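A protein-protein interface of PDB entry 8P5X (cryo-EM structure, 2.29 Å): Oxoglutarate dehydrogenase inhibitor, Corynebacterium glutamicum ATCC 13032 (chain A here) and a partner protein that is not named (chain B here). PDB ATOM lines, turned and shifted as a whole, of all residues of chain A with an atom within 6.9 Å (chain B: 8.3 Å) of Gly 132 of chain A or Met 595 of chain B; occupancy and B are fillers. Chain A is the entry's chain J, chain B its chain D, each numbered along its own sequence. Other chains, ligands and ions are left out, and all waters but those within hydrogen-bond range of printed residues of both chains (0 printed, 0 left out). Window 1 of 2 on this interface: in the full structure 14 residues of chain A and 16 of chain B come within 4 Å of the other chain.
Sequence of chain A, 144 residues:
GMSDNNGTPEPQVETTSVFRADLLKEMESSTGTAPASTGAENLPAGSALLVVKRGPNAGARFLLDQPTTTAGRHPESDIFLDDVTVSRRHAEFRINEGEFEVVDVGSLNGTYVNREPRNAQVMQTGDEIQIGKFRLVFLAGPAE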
ATOM      1  N   ARG A  54     -38.256 -16.330   1.023  1.00  0.00           N
ATOM      2  CA  ARG A  54     -38.123 -17.684   0.417  1.00  0.00           C
ATOM      3  C   ARG A  54     -37.022 -18.463   1.138  1.00  0.00           C
ATOM      4  O   ARG A  54     -35.920 -17.909   1.287  1.00  0.00           O
ATOM      5  CB  ARG A  54     -37.774 -17.544  -1.065  1.00  0.00           C
ATOM      6  CG  ARG A  54     -38.007 -18.799  -1.891  1.00  0.00           C
ATOM      7  CD  ARG A  54     -37.174 -18.769  -3.157  1.00  0.00           C
ATOM      8  NE  ARG A  54     -37.648 -19.691  -4.179  1.00  0.00           N
ATOM      9  CZ  ARG A  54     -36.966 -20.061  -5.263  1.00  0.00           C
ATOM     10  NH1 ARG A  54     -35.742 -19.604  -5.492  1.00  0.00           N
ATOM     11  NH2 ARG A  54     -37.514 -20.905  -6.121  1.00  0.00           N
ATOM     12  N   ASP A  83     -27.706 -24.209   5.552  1.00  0.00           N
ATOM     13  CA  ASP A  83     -27.860 -24.855   4.223  1.00  0.00           C
ATOM     14  C   ASP A  83     -26.477 -25.008   3.587  1.00  0.00           C
ATOM     15  O   ASP A  83     -25.578 -24.211   3.919  1.00  0.00           O
ATOM     16  CB  ASP A  83     -28.792 -24.053   3.316  1.00  0.00           C
ATOM     17  CG  ASP A  83     -29.238 -24.794   2.062  1.00  0.00           C
ATOM     18  OD1 ASP A  83     -29.673 -25.962   2.190  1.00  0.00           O
ATOM     19  OD2 ASP A  83     -29.151 -24.199   0.963  1.00  0.00           O
ATOM     20  N   THR A  85     -25.512 -24.347   0.614  1.00  0.00           N
ATOM     21  CA  THR A  85     -25.214 -23.234  -0.320  1.00  0.00           C
ATOM     22  C   THR A  85     -24.626 -22.034   0.416  1.00  0.00           C
ATOM     23  O   THR A  85     -23.982 -21.228  -0.258  1.00  0.00           O
ATOM     24  CB  THR A  85     -26.458 -22.830  -1.106  1.00  0.00           C
ATOM     25  OG1 THR A  85     -27.467 -22.441  -0.173  1.00  0.00           O
ATOM     26  CG2 THR A  85     -26.974 -23.943  -1.986  1.00  0.00           C
ATOM     27  N   VAL A  86     -24.829 -21.907   1.724  1.00  0.00           N
ATOM     28  CA  VAL A  86     -24.290 -20.787   2.547  1.00  0.00           C
ATOM     29  C   VAL A  86     -22.926 -21.188   3.110  1.00  0.00           C
ATOM     30  O   VAL A  86     -22.787 -22.346   3.549  1.00  0.00           O
ATOM     31  CB  VAL A  86     -25.253 -20.416   3.679  1.00  0.00           C
ATOM     32  CG1 VAL A  86     -24.705 -19.281   4.524  1.00  0.00           C
ATOM     33  CG2 VAL A  86     -26.626 -20.071   3.143  1.00  0.00           C
ATOM     34  N   HIS A  90     -20.145 -15.525   5.491  1.00  0.00           N
ATOM     35  CA  HIS A  90     -20.749 -15.244   4.155  1.00  0.00           C
ATOM     36  C   HIS A  90     -20.951 -13.759   3.904  1.00  0.00           C
ATOM     37  O   HIS A  90     -20.553 -13.312   2.815  1.00  0.00           O
ATOM     38  CB  HIS A  90     -22.067 -15.971   3.966  1.00  0.00           C
ATOM     39  CG  HIS A  90     -22.504 -16.080   2.547  1.00  0.00           C
ATOM     40  ND1 HIS A  90     -22.678 -17.272   1.934  1.00  0.00           N
ATOM     41  CD2 HIS A  90     -22.851 -15.156   1.639  1.00  0.00           C
ATOM     42  CE1 HIS A  90     -23.091 -17.084   0.705  1.00  0.00           C
ATOM     43  NE2 HIS A  90     -23.200 -15.803   0.496  1.00  0.00           N
ATOM     44  N   ASN A 109     -20.373 -18.626  -3.429  1.00  0.00           N
ATOM     45  CA  ASN A 109     -21.533 -18.344  -4.308  1.00  0.00           C
ATOM     46  C   ASN A 109     -21.768 -16.839  -4.442  1.00  0.00           C
ATOM     47  O   ASN A 109     -22.459 -16.450  -5.395  1.00  0.00           O
ATOM     48  CB  ASN A 109     -22.792 -19.048  -3.813  1.00  0.00           C
ATOM     49  CG  ASN A 109     -22.828 -20.527  -4.126  1.00  0.00           C
ATOM     50  OD1 ASN A 109     -22.340 -20.966  -5.159  1.00  0.00           O
ATOM     51  ND2 ASN A 109     -23.438 -21.304  -3.250  1.00  0.00           N
ATOM     52  N   GLY A 110     -21.251 -16.023  -3.533  1.00  0.00           N
ATOM     53  CA  GLY A 110     -21.391 -14.561  -3.587  1.00  0.00           C
ATOM     54  C   GLY A 110     -22.727 -14.096  -3.061  1.00  0.00           C
ATOM     55  O   GLY A 110     -23.567 -14.952  -2.769  1.00  0.00           O
ATOM     56  N   THR A 111     -22.907 -12.778  -2.949  1.00  0.00           N
ATOM     57  CA  THR A 111     -24.152 -12.087  -2.526  1.00  0.00           C
ATOM     58  C   THR A 111     -24.745 -11.311  -3.699  1.00  0.00           C
ATOM     59  O   THR A 111     -23.978 -10.615  -4.374  1.00  0.00           O
ATOM     60  CB  THR A 111     -23.854 -11.115  -1.394  1.00  0.00           C
ATOM     61  OG1 THR A 111     -23.150 -11.837  -0.387  1.00  0.00           O
ATOM     62  CG2 THR A 111     -25.100 -10.510  -0.799  1.00  0.00           C
ATOM     63  N   TYR A 112     -26.060 -11.414  -3.916  1.00  0.00           N
ATOM     64  CA  TYR A 112     -26.832 -10.706  -4.969  1.00  0.00           C
ATOM     65  C   TYR A 112     -27.807  -9.714  -4.335  1.00  0.00           C
ATOM     66  O   TYR A 112     -28.494 -10.112  -3.390  1.00  0.00           O
ATOM     67  CB  TYR A 112     -27.639 -11.702  -5.787  1.00  0.00           C
ATOM     68  CG  TYR A 112     -26.832 -12.668  -6.611  1.00  0.00           C
ATOM     69  CD1 TYR A 112     -26.331 -13.828  -6.062  1.00  0.00           C
ATOM     70  CD2 TYR A 112     -26.609 -12.447  -7.953  1.00  0.00           C
ATOM     71  CE1 TYR A 112     -25.604 -14.732  -6.817  1.00  0.00           C
ATOM     72  CE2 TYR A 112     -25.888 -13.341  -8.724  1.00  0.00           C
ATOM     73  CZ  TYR A 112     -25.385 -14.490  -8.155  1.00  0.00           C
ATOM     74  OH  TYR A 112     -24.669 -15.378  -8.904  1.00  0.00           O
ATOM     75  N   GLN A 130     -29.994 -11.969  -1.691  1.00  0.00           N
ATOM     76  CA  GLN A 130     -29.860 -13.440  -1.843  1.00  0.00           C
ATOM     77  C   GLN A 130     -28.530 -13.914  -1.249  1.00  0.00           C
ATOM     78  O   GLN A 130     -27.471 -13.446  -1.715  1.00  0.00           O
ATOM     79  CB  GLN A 130     -29.951 -13.835  -3.307  1.00  0.00           C
ATOM     80  CG  GLN A 130     -30.308 -15.298  -3.499  1.00  0.00           C
ATOM     81  CD  GLN A 130     -30.358 -15.704  -4.948  1.00  0.00           C
ATOM     82  OE1 GLN A 130     -30.532 -14.880  -5.842  1.00  0.00           O
ATOM     83  NE2 GLN A 130     -30.212 -16.995  -5.189  1.00  0.00           N
ATOM     84  N   ILE A 131     -28.599 -14.792  -0.243  1.00  0.00           N
ATOM     85  CA  ILE A 131     -27.466 -15.521   0.388  1.00  0.00           C
ATOM     86  C   ILE A 131     -27.758 -17.008   0.245  1.00  0.00           C
ATOM     87  O   ILE A 131     -28.517 -17.537   1.060  1.00  0.00           O
ATOM     88  CB  ILE A 131     -27.317 -15.127   1.860  1.00  0.00           C
ATOM     89  CG1 ILE A 131     -27.031 -13.642   2.021  1.00  0.00           C
ATOM     90  CG2 ILE A 131     -26.253 -15.970   2.536  1.00  0.00           C
ATOM     91  CD1 ILE A 131     -27.138 -13.164   3.435  1.00  0.00           C
ATOM     92  N   GLY A 132     -27.218 -17.646  -0.782  1.00  0.00           N
ATOM     93  CA  GLY A 132     -27.439 -19.069  -1.067  1.00  0.00           C
ATOM     94  C   GLY A 132     -28.772 -19.277  -1.737  1.00  0.00           C
ATOM     95  O   GLY A 132     -28.987 -18.666  -2.794  1.00  0.00           O
ATOM     96  N   LYS A 133     -29.629 -20.108  -1.144  1.00  0.00           N
ATOM     97  CA  LYS A 133     -31.020 -20.344  -1.588  1.00  0.00           C
ATOM     98  C   LYS A 133     -31.993 -19.530  -0.734  1.00  0.00           C
ATOM     99  O   LYS A 133     -33.202 -19.591  -1.028  1.00  0.00           O
ATOM    100  CB  LYS A 133     -31.336 -21.838  -1.545  1.00  0.00           C
ATOM    101  CG  LYS A 133     -30.614 -22.651  -2.605  1.00  0.00           C
ATOM    102  CD  LYS A 133     -31.211 -24.011  -2.852  1.00  0.00           C
ATOM    103  CE  LYS A 133     -30.612 -24.684  -4.070  1.00  0.00           C
ATOM    104  NZ  LYS A 133     -31.139 -26.059  -4.255  1.00  0.00           N
ATOM    105  N   PHE A 134     -31.512 -18.792   0.268  1.00  0.00           N
ATOM    106  CA  PHE A 134     -32.344 -17.885   1.091  1.00  0.00           C
ATOM    107  C   PHE A 134     -32.476 -16.554   0.363  1.00  0.00           C
ATOM    108  O   PHE A 134     -31.472 -16.105  -0.218  1.00  0.00           O
ATOM    109  CB  PHE A 134     -31.741 -17.661   2.470  1.00  0.00           C
ATOM    110  CG  PHE A 134     -31.702 -18.875   3.353  1.00  0.00           C
ATOM    111  CD1 PHE A 134     -30.664 -19.779   3.261  1.00  0.00           C
ATOM    112  CD2 PHE A 134     -32.677 -19.101   4.296  1.00  0.00           C
ATOM    113  CE1 PHE A 134     -30.609 -20.888   4.085  1.00  0.00           C
ATOM    114  CE2 PHE A 134     -32.622 -20.211   5.117  1.00  0.00           C
ATOM    115  CZ  PHE A 134     -31.590 -21.101   5.011  1.00  0.00           C
ATOM    116  N   ARG A 135     -33.678 -15.968   0.381  1.00  0.00           N
ATOM    117  CA  ARG A 135     -33.988 -14.614  -0.145  1.00  0.00           C
ATOM    118  C   ARG A 135     -34.654 -13.812   0.967  1.00  0.00           C
ATOM    119  O   ARG A 135     -35.625 -14.322   1.544  1.00  0.00           O
ATOM    120  CB  ARG A 135     -34.875 -14.721  -1.383  1.00  0.00           C
ATOM    121  CG  ARG A 135     -34.092 -15.018  -2.650  1.00  0.00           C
ATOM    122  CD  ARG A 135     -34.946 -15.531  -3.787  1.00  0.00           C
ATOM    123  NE  ARG A 135     -34.123 -15.952  -4.912  1.00  0.00           N
ATOM    124  CZ  ARG A 135     -34.581 -16.463  -6.053  1.00  0.00           C
ATOM    125  NH1 ARG A 135     -35.882 -16.621  -6.254  1.00  0.00           N
ATOM    126  NH2 ARG A 135     -33.726 -16.821  -6.999  1.00  0.00           N
ATOM    127  N   ALA B 483     -20.127 -18.996 -12.215  1.00  0.00           N
ATOM    128  CA  ALA B 483     -21.087 -19.254 -11.131  1.00  0.00           C
ATOM    129  C   ALA B 483     -21.581 -20.686 -11.214  1.00  0.00           C
ATOM    130  O   ALA B 483     -21.590 -21.362 -10.176  1.00  0.00           O
ATOM    131  CB  ALA B 483     -22.225 -18.292 -11.223  1.00  0.00           C
ATOM    132  N   GLU B 484     -21.976 -21.135 -12.398  1.00  0.00           N
ATOM    133  CA  GLU B 484     -22.463 -22.509 -12.638  1.00  0.00           C
ATOM    134  C   GLU B 484     -21.382 -23.498 -12.227  1.00  0.00           C
ATOM    135  O   GLU B 484     -21.713 -24.476 -11.528  1.00  0.00           O
ATOM    136  CB  GLU B 484     -22.831 -22.710 -14.102  1.00  0.00           C
ATOM    137  CG  GLU B 484     -24.158 -22.082 -14.480  1.00  0.00           C
ATOM    138  CD  GLU B 484     -24.404 -21.947 -15.977  1.00  0.00           C
ATOM    139  OE1 GLU B 484     -23.857 -22.772 -16.750  1.00  0.00           O
ATOM    140  OE2 GLU B 484     -25.137 -21.009 -16.372  1.00  0.00           O
ATOM    141  N   LYS B 486     -18.867 -23.217 -10.111  1.00  0.00           N
ATOM    142  CA  LYS B 486     -18.622 -23.280  -8.660  1.00  0.00           C
ATOM    143  C   LYS B 486     -19.750 -24.003  -7.948  1.00  0.00           C
ATOM    144  O   LYS B 486     -19.466 -24.614  -6.915  1.00  0.00           O
ATOM    145  CB  LYS B 486     -18.464 -21.892  -8.075  1.00  0.00           C
ATOM    146  CG  LYS B 486     -17.252 -21.147  -8.581  1.00  0.00           C
ATOM    147  CD  LYS B 486     -16.920 -19.963  -7.738  1.00  0.00           C
ATOM    148  CE  LYS B 486     -16.503 -18.776  -8.558  1.00  0.00           C
ATOM    149  NZ  LYS B 486     -16.539 -17.550  -7.729  1.00  0.00           N
ATOM    150  N   TYR B 487     -20.965 -23.971  -8.466  1.00  0.00           N
ATOM    151  CA  TYR B 487     -22.123 -24.682  -7.884  1.00  0.00           C
ATOM    152  C   TYR B 487     -21.940 -26.188  -8.066  1.00  0.00           C
ATOM    153  O   TYR B 487     -22.349 -26.925  -7.155  1.00  0.00           O
ATOM    154  CB  TYR B 487     -23.426 -24.142  -8.472  1.00  0.00           C
ATOM    155  CG  TYR B 487     -24.679 -24.741  -7.889  1.00  0.00           C
ATOM    156  CD1 TYR B 487     -25.172 -24.323  -6.679  1.00  0.00           C
ATOM    157  CD2 TYR B 487     -25.356 -25.746  -8.543  1.00  0.00           C
ATOM    158  CE1 TYR B 487     -26.305 -24.889  -6.126  1.00  0.00           C
ATOM    159  CE2 TYR B 487     -26.491 -26.324  -8.009  1.00  0.00           C
ATOM    160  CZ  TYR B 487     -26.965 -25.897  -6.791  1.00  0.00           C
ATOM    161  OH  TYR B 487     -28.092 -26.460  -6.259  1.00  0.00           O
ATOM    162  N   GLN B 490     -19.386 -27.355  -5.401  1.00  0.00           N
ATOM    163  CA  GLN B 490     -19.940 -27.363  -4.032  1.00  0.00           C
ATOM    164  C   GLN B 490     -20.736 -28.640  -3.799  1.00  0.00           C
ATOM    165  O   GLN B 490     -20.694 -29.132  -2.666  1.00  0.00           O
ATOM    166  CB  GLN B 490     -20.792 -26.126  -3.822  1.00  0.00           C
ATOM    167  CG  GLN B 490     -21.042 -25.810  -2.368  1.00  0.00           C
ATOM    168  CD  GLN B 490     -21.647 -24.445  -2.212  1.00  0.00           C
ATOM    169  OE1 GLN B 490     -22.465 -24.014  -3.016  1.00  0.00           O
ATOM    170  NE2 GLN B 490     -21.257 -23.753  -1.158  1.00  0.00           N
ATOM    171  N   ASP B 525     -29.525 -33.766  -9.352  1.00  0.00           N
ATOM    172  CA  ASP B 525     -29.821 -32.348  -9.043  1.00  0.00           C
ATOM    173  C   ASP B 525     -30.161 -31.598 -10.322  1.00  0.00           C
ATOM    174  O   ASP B 525     -31.039 -30.733 -10.270  1.00  0.00           O
ATOM    175  CB  ASP B 525     -28.647 -31.683  -8.336  1.00  0.00           C
ATOM    176  CG  ASP B 525     -28.970 -30.341  -7.706  1.00  0.00           C
ATOM    177  OD1 ASP B 525     -29.997 -30.257  -6.993  1.00  0.00           O
ATOM    178  OD2 ASP B 525     -28.184 -29.385  -7.918  1.00  0.00           O
ATOM    179  N   ASP B 529     -33.881 -29.852 -11.070  1.00  0.00           N
ATOM    180  CA  ASP B 529     -33.868 -28.384 -11.259  1.00  0.00           C
ATOM    181  C   ASP B 529     -34.517 -28.030 -12.592  1.00  0.00           C
ATOM    182  O   ASP B 529     -35.243 -27.028 -12.636  1.00  0.00           O
ATOM    183  CB  ASP B 529     -32.454 -27.834 -11.184  1.00  0.00           C
ATOM    184  CG  ASP B 529     -32.413 -26.335 -10.983  1.00  0.00           C
ATOM    185  OD1 ASP B 529     -32.700 -25.896  -9.848  1.00  0.00           O
ATOM    186  OD2 ASP B 529     -32.100 -25.618 -11.962  1.00  0.00           O
ATOM    187  N   ALA B 532     -38.302 -28.232 -12.273  1.00  0.00           N
ATOM    188  CA  ALA B 532     -38.817 -27.071 -11.525  1.00  0.00           C
ATOM    189  C   ALA B 532     -38.978 -25.873 -12.449  1.00  0.00           C
ATOM    190  O   ALA B 532     -39.911 -25.095 -12.242  1.00  0.00           O
ATOM    191  CB  ALA B 532     -37.901 -26.750 -10.390  1.00  0.00           C
ATOM    192  N   HIS B 592     -37.478 -28.753  -2.975  1.00  0.00           N
ATOM    193  CA  HIS B 592     -36.297 -28.321  -3.758  1.00  0.00           C
ATOM    194  C   HIS B 592     -36.551 -26.947  -4.341  1.00  0.00           C
ATOM    195  O   HIS B 592     -37.367 -26.849  -5.263  1.00  0.00           O
ATOM    196  CB  HIS B 592     -36.000 -29.298  -4.880  1.00  0.00           C
ATOM    197  CG  HIS B 592     -34.815 -28.945  -5.710  1.00  0.00           C
ATOM    198  ND1 HIS B 592     -34.874 -28.068  -6.747  1.00  0.00           N
ATOM    199  CD2 HIS B 592     -33.550 -29.396  -5.692  1.00  0.00           C
ATOM    200  CE1 HIS B 592     -33.693 -27.976  -7.313  1.00  0.00           C
ATOM    201  NE2 HIS B 592     -32.872 -28.771  -6.690  1.00  0.00           N
ATOM    202  N   LEU B 593     -35.873 -25.930  -3.816  1.00  0.00           N
ATOM    203  CA  LEU B 593     -35.858 -24.552  -4.352  1.00  0.00           C
ATOM    204  C   LEU B 593     -34.797 -24.492  -5.431  1.00  0.00           C
ATOM    205  O   LEU B 593     -33.939 -25.378  -5.463  1.00  0.00           O
ATOM    206  CB  LEU B 593     -35.554 -23.581  -3.223  1.00  0.00           C
ATOM    207  CG  LEU B 593     -36.735 -23.208  -2.352  1.00  0.00           C
ATOM    208  CD1 LEU B 593     -37.421 -24.434  -1.802  1.00  0.00           C
ATOM    209  CD2 LEU B 593     -36.294 -22.321  -1.220  1.00  0.00           C
ATOM    210  N   GLN B 594     -34.861 -23.480  -6.281  1.00  0.00           N
ATOM    211  CA  GLN B 594     -34.052 -23.329  -7.510  1.00  0.00           C
ATOM    212  C   GLN B 594     -33.144 -22.113  -7.317  1.00  0.00           C
ATOM    213  O   GLN B 594     -33.679 -21.006  -7.157  1.00  0.00           O
ATOM    214  CB  GLN B 594     -35.042 -23.202  -8.662  1.00  0.00           C
ATOM    215  CG  GLN B 594     -34.425 -23.162 -10.043  1.00  0.00           C
ATOM    216  CD  GLN B 594     -35.467 -23.236 -11.126  1.00  0.00           C
ATOM    217  OE1 GLN B 594     -36.520 -22.618 -11.045  1.00  0.00           O
ATOM    218  NE2 GLN B 594     -35.178 -23.987 -12.170  1.00  0.00           N
ATOM    219  N   MET B 595     -31.826 -22.321  -7.333  1.00  0.00           N
ATOM    220  CA  MET B 595     -30.762 -21.334  -7.005  1.00  0.00           C
ATOM    221  C   MET B 595     -30.874 -20.098  -7.891  1.00  0.00           C
ATOM    222  O   MET B 595     -30.889 -18.991  -7.345  1.00  0.00           O
ATOM    223  CB  MET B 595     -29.391 -21.980  -7.225  1.00  0.00           C
ATOM    224  CG  MET B 595     -28.197 -21.086  -6.939  1.00  0.00           C
ATOM    225  SD  MET B 595     -27.969 -20.817  -5.189  1.00  0.00           S
ATOM    226  CE  MET B 595     -26.361 -20.032  -5.195  1.00  0.00           C
ATOM    227  N   PHE B 596     -30.922 -20.291  -9.207  1.00  0.00           N
ATOM    228  CA  PHE B 596     -30.911 -19.226 -10.236  1.00  0.00           C
ATOM    229  C   PHE B 596     -32.255 -19.195 -10.964  1.00  0.00           C
ATOM    230  O   PHE B 596     -32.279 -19.266 -12.206  1.00  0.00           O
ATOM    231  CB  PHE B 596     -29.774 -19.481 -11.225  1.00  0.00           C
ATOM    232  CG  PHE B 596     -28.399 -19.615 -10.621  1.00  0.00           C
ATOM    233  CD1 PHE B 596     -27.843 -18.582  -9.886  1.00  0.00           C
ATOM    234  CD2 PHE B 596     -27.646 -20.762 -10.820  1.00  0.00           C
ATOM    235  CE1 PHE B 596     -26.574 -18.705  -9.344  1.00  0.00           C
ATOM    236  CE2 PHE B 596     -26.377 -20.883 -10.279  1.00  0.00           C
ATOM    237  CZ  PHE B 596     -25.844 -19.854  -9.546  1.00  0.00           C
ATOM    238  N   GLY B 597     -33.354 -19.093 -10.221  1.00  0.00           N
ATOM    239  CA  GLY B 597     -34.715 -19.052 -10.778  1.00  0.00           C
ATOM    240  C   GLY B 597     -35.730 -18.775  -9.699  1.00  0.00           C
ATOM    241  O   GLY B 597     -35.305 -18.410  -8.602  1.00  0.00           O
ATOM    242  N   ASP B 598     -37.017 -18.969  -9.980  1.00  0.00           N
ATOM    243  CA  ASP B 598     -38.108 -18.771  -8.999  1.00  0.00           C
ATOM    244  C   ASP B 598     -38.979 -20.024  -8.889  1.00  0.00           C
ATOM    245  O   ASP B 598     -40.121 -19.889  -8.436  1.00  0.00           O
ATOM    246  CB  ASP B 598     -38.926 -17.543  -9.380  1.00  0.00           C
ATOM    247  CG  ASP B 598     -38.082 -16.293  -9.566  1.00  0.00           C
ATOM    248  OD1 ASP B 598     -37.184 -16.055  -8.721  1.00  0.00           O
ATOM    249  OD2 ASP B 598     -38.322 -15.564 -10.560  1.00  0.00           O
ATOM    250  N   GLY B 599     -38.452 -21.206  -9.209  1.00  0.00           N
ATOM    251  CA  GLY B 599     -39.202 -22.473  -9.194  1.00  0.00           C
ATOM    252  C   GLY B 599     -39.017 -23.247  -7.906  1.00  0.00           C
ATOM    253  O   GLY B 599     -37.911 -23.203  -7.354  1.00  0.00           O
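O of Asp 529 of chain B sits at hydrogen-bond distance from NE2 of Gln 594 of chain B (3.1 Å). The side-chain carboxylate (OD2) of Asp 83 of chain A lies within hydrogen-bond range of the side-chain hydroxyl (OG1) of Thr 85 of chain A (2.7 Å). O of Thr 85 of chain A is in hydrogen-bond range of ND2 of Asn 109 of chain A (3.0 Å). The backbone NH (N) of Lys 133 of chain A is in hydrogen-bond range of the side-chain hydroxyl (OG1) of Thr 85 of chain A (3.3 Å). The backbone carbonyl oxygen (O) of Tyr 112 of chain A lies within hydrogen-bond range of the backbone NH (N) of Gln 130 of chain A (2.9 Å). The side-chain amide nitrogen (NE2) of Gln 130 of chain A lies within hydrogen-bond range of the backbone carbonyl oxygen (O) of Gly 132 of chain A, at 3.2 Å.
Ile 131 of chain A touches none of the printed residues of chain B. Gly 132 of chain A touches just one residue of chain B: Met 595 (3.4 Å). Printed residues of chain B within 4 Å of Arg 135 of chain A: Met 595, Gly 597 and Asp 598. His 592 of chain B touches none of the printed residues of chain A. Of the printed residues of chain A, Gln 594 of chain B touches Arg 54. Of chain A, only Asn 109, Gln 130, Gly 132 and Arg 135 come within 4 Å of Met 595 of chain B. The nearest residue of chain A that does not touch Met 595 of chain B is Lys 133 of chain A (4.1 Å). The nearest printed residue of chain A that does not touch Gly 597 of chain B is Gln 130 of chain A (6.3 Å).
CG of Arg 54 of chain A touches CD2 of Leu 593 of chain B (3.97 Å). Arg 54 of chain A touches Asp 598 of chain B (NH2 to C, 3.3 Å). Gln 490 of chain B touches Thr 85 of chain A (NE2 to O, 3.8 Å). CG of Asn 109 of chain A touches CE of Met 595 of chain B, at 3.7 Å. Tyr 112 of chain A touches Phe 596 of chain B. NZ of Lys 133 of chain A touches OH of Tyr 487 of chain B (3.7 Å). NH2 of Arg 135 of chain A touches O of Met 595 of chain B, 3.6 Å away.
The side-chain amide nitrogen of Asn 109 of chain A lies within hydrogen-bond range of the side-chain amide oxygen of Gln 490 of chain B (2.9 Å). The side-chain amino group of Lys 133 of chain A sits at hydrogen-bond distance from the backbone carbonyl oxygen of Leu 593 of chain B (3.1 Å). The backbone carbonyl oxygen (O) of Gln 594 of chain B is in hydrogen-bond range of the guanidinium group (NH1) of Arg 54 of chain A (3.0 Å). The backbone carbonyl oxygen of Met 595 of chain B lies within hydrogen-bond range of the side-chain amide nitrogen of Gln 130 of chain A, 3.0 Å away. The backbone carbonyl oxygen of Gly 597 of chain B lies within hydrogen-bond range of the guanidinium group of Arg 54 of chain A (3.4 Å). O of Gly 597 of chain B sits at hydrogen-bond distance from NH2 of Arg 135 of chain A (2.8 Å). The side-chain carboxylate of Asp 598 of chain B is in salt-bridge range of the guanidinium group of Arg 135 of chain A (2.8 Å). O of Gly 599 of chain B sits at hydrogen-bond distance from NH2 of Arg 54 of chain A, 2.6 Å away. The backbone carbonyl oxygen (O) of Gly 132 of chain A lies close to the side-chain sulfur (SD) of Met 595 of chain B, 3.4 Å away.
Hydrophobic or aromatic side chains of chain B within 4 Å of the printed part of chain A: Tyr 487, Leu 593, Met 595 and Phe 596. Hydrophobic or aromatic side chains of chain A within 4 Å of the printed part of chain B: Tyr 112. Among the printed residues, Asp or Glu carboxylates within 4 Å of a Lys or Arg side-chain nitrogen of the other chain: Arg 135 of chain A with Asp 598 of chain B.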
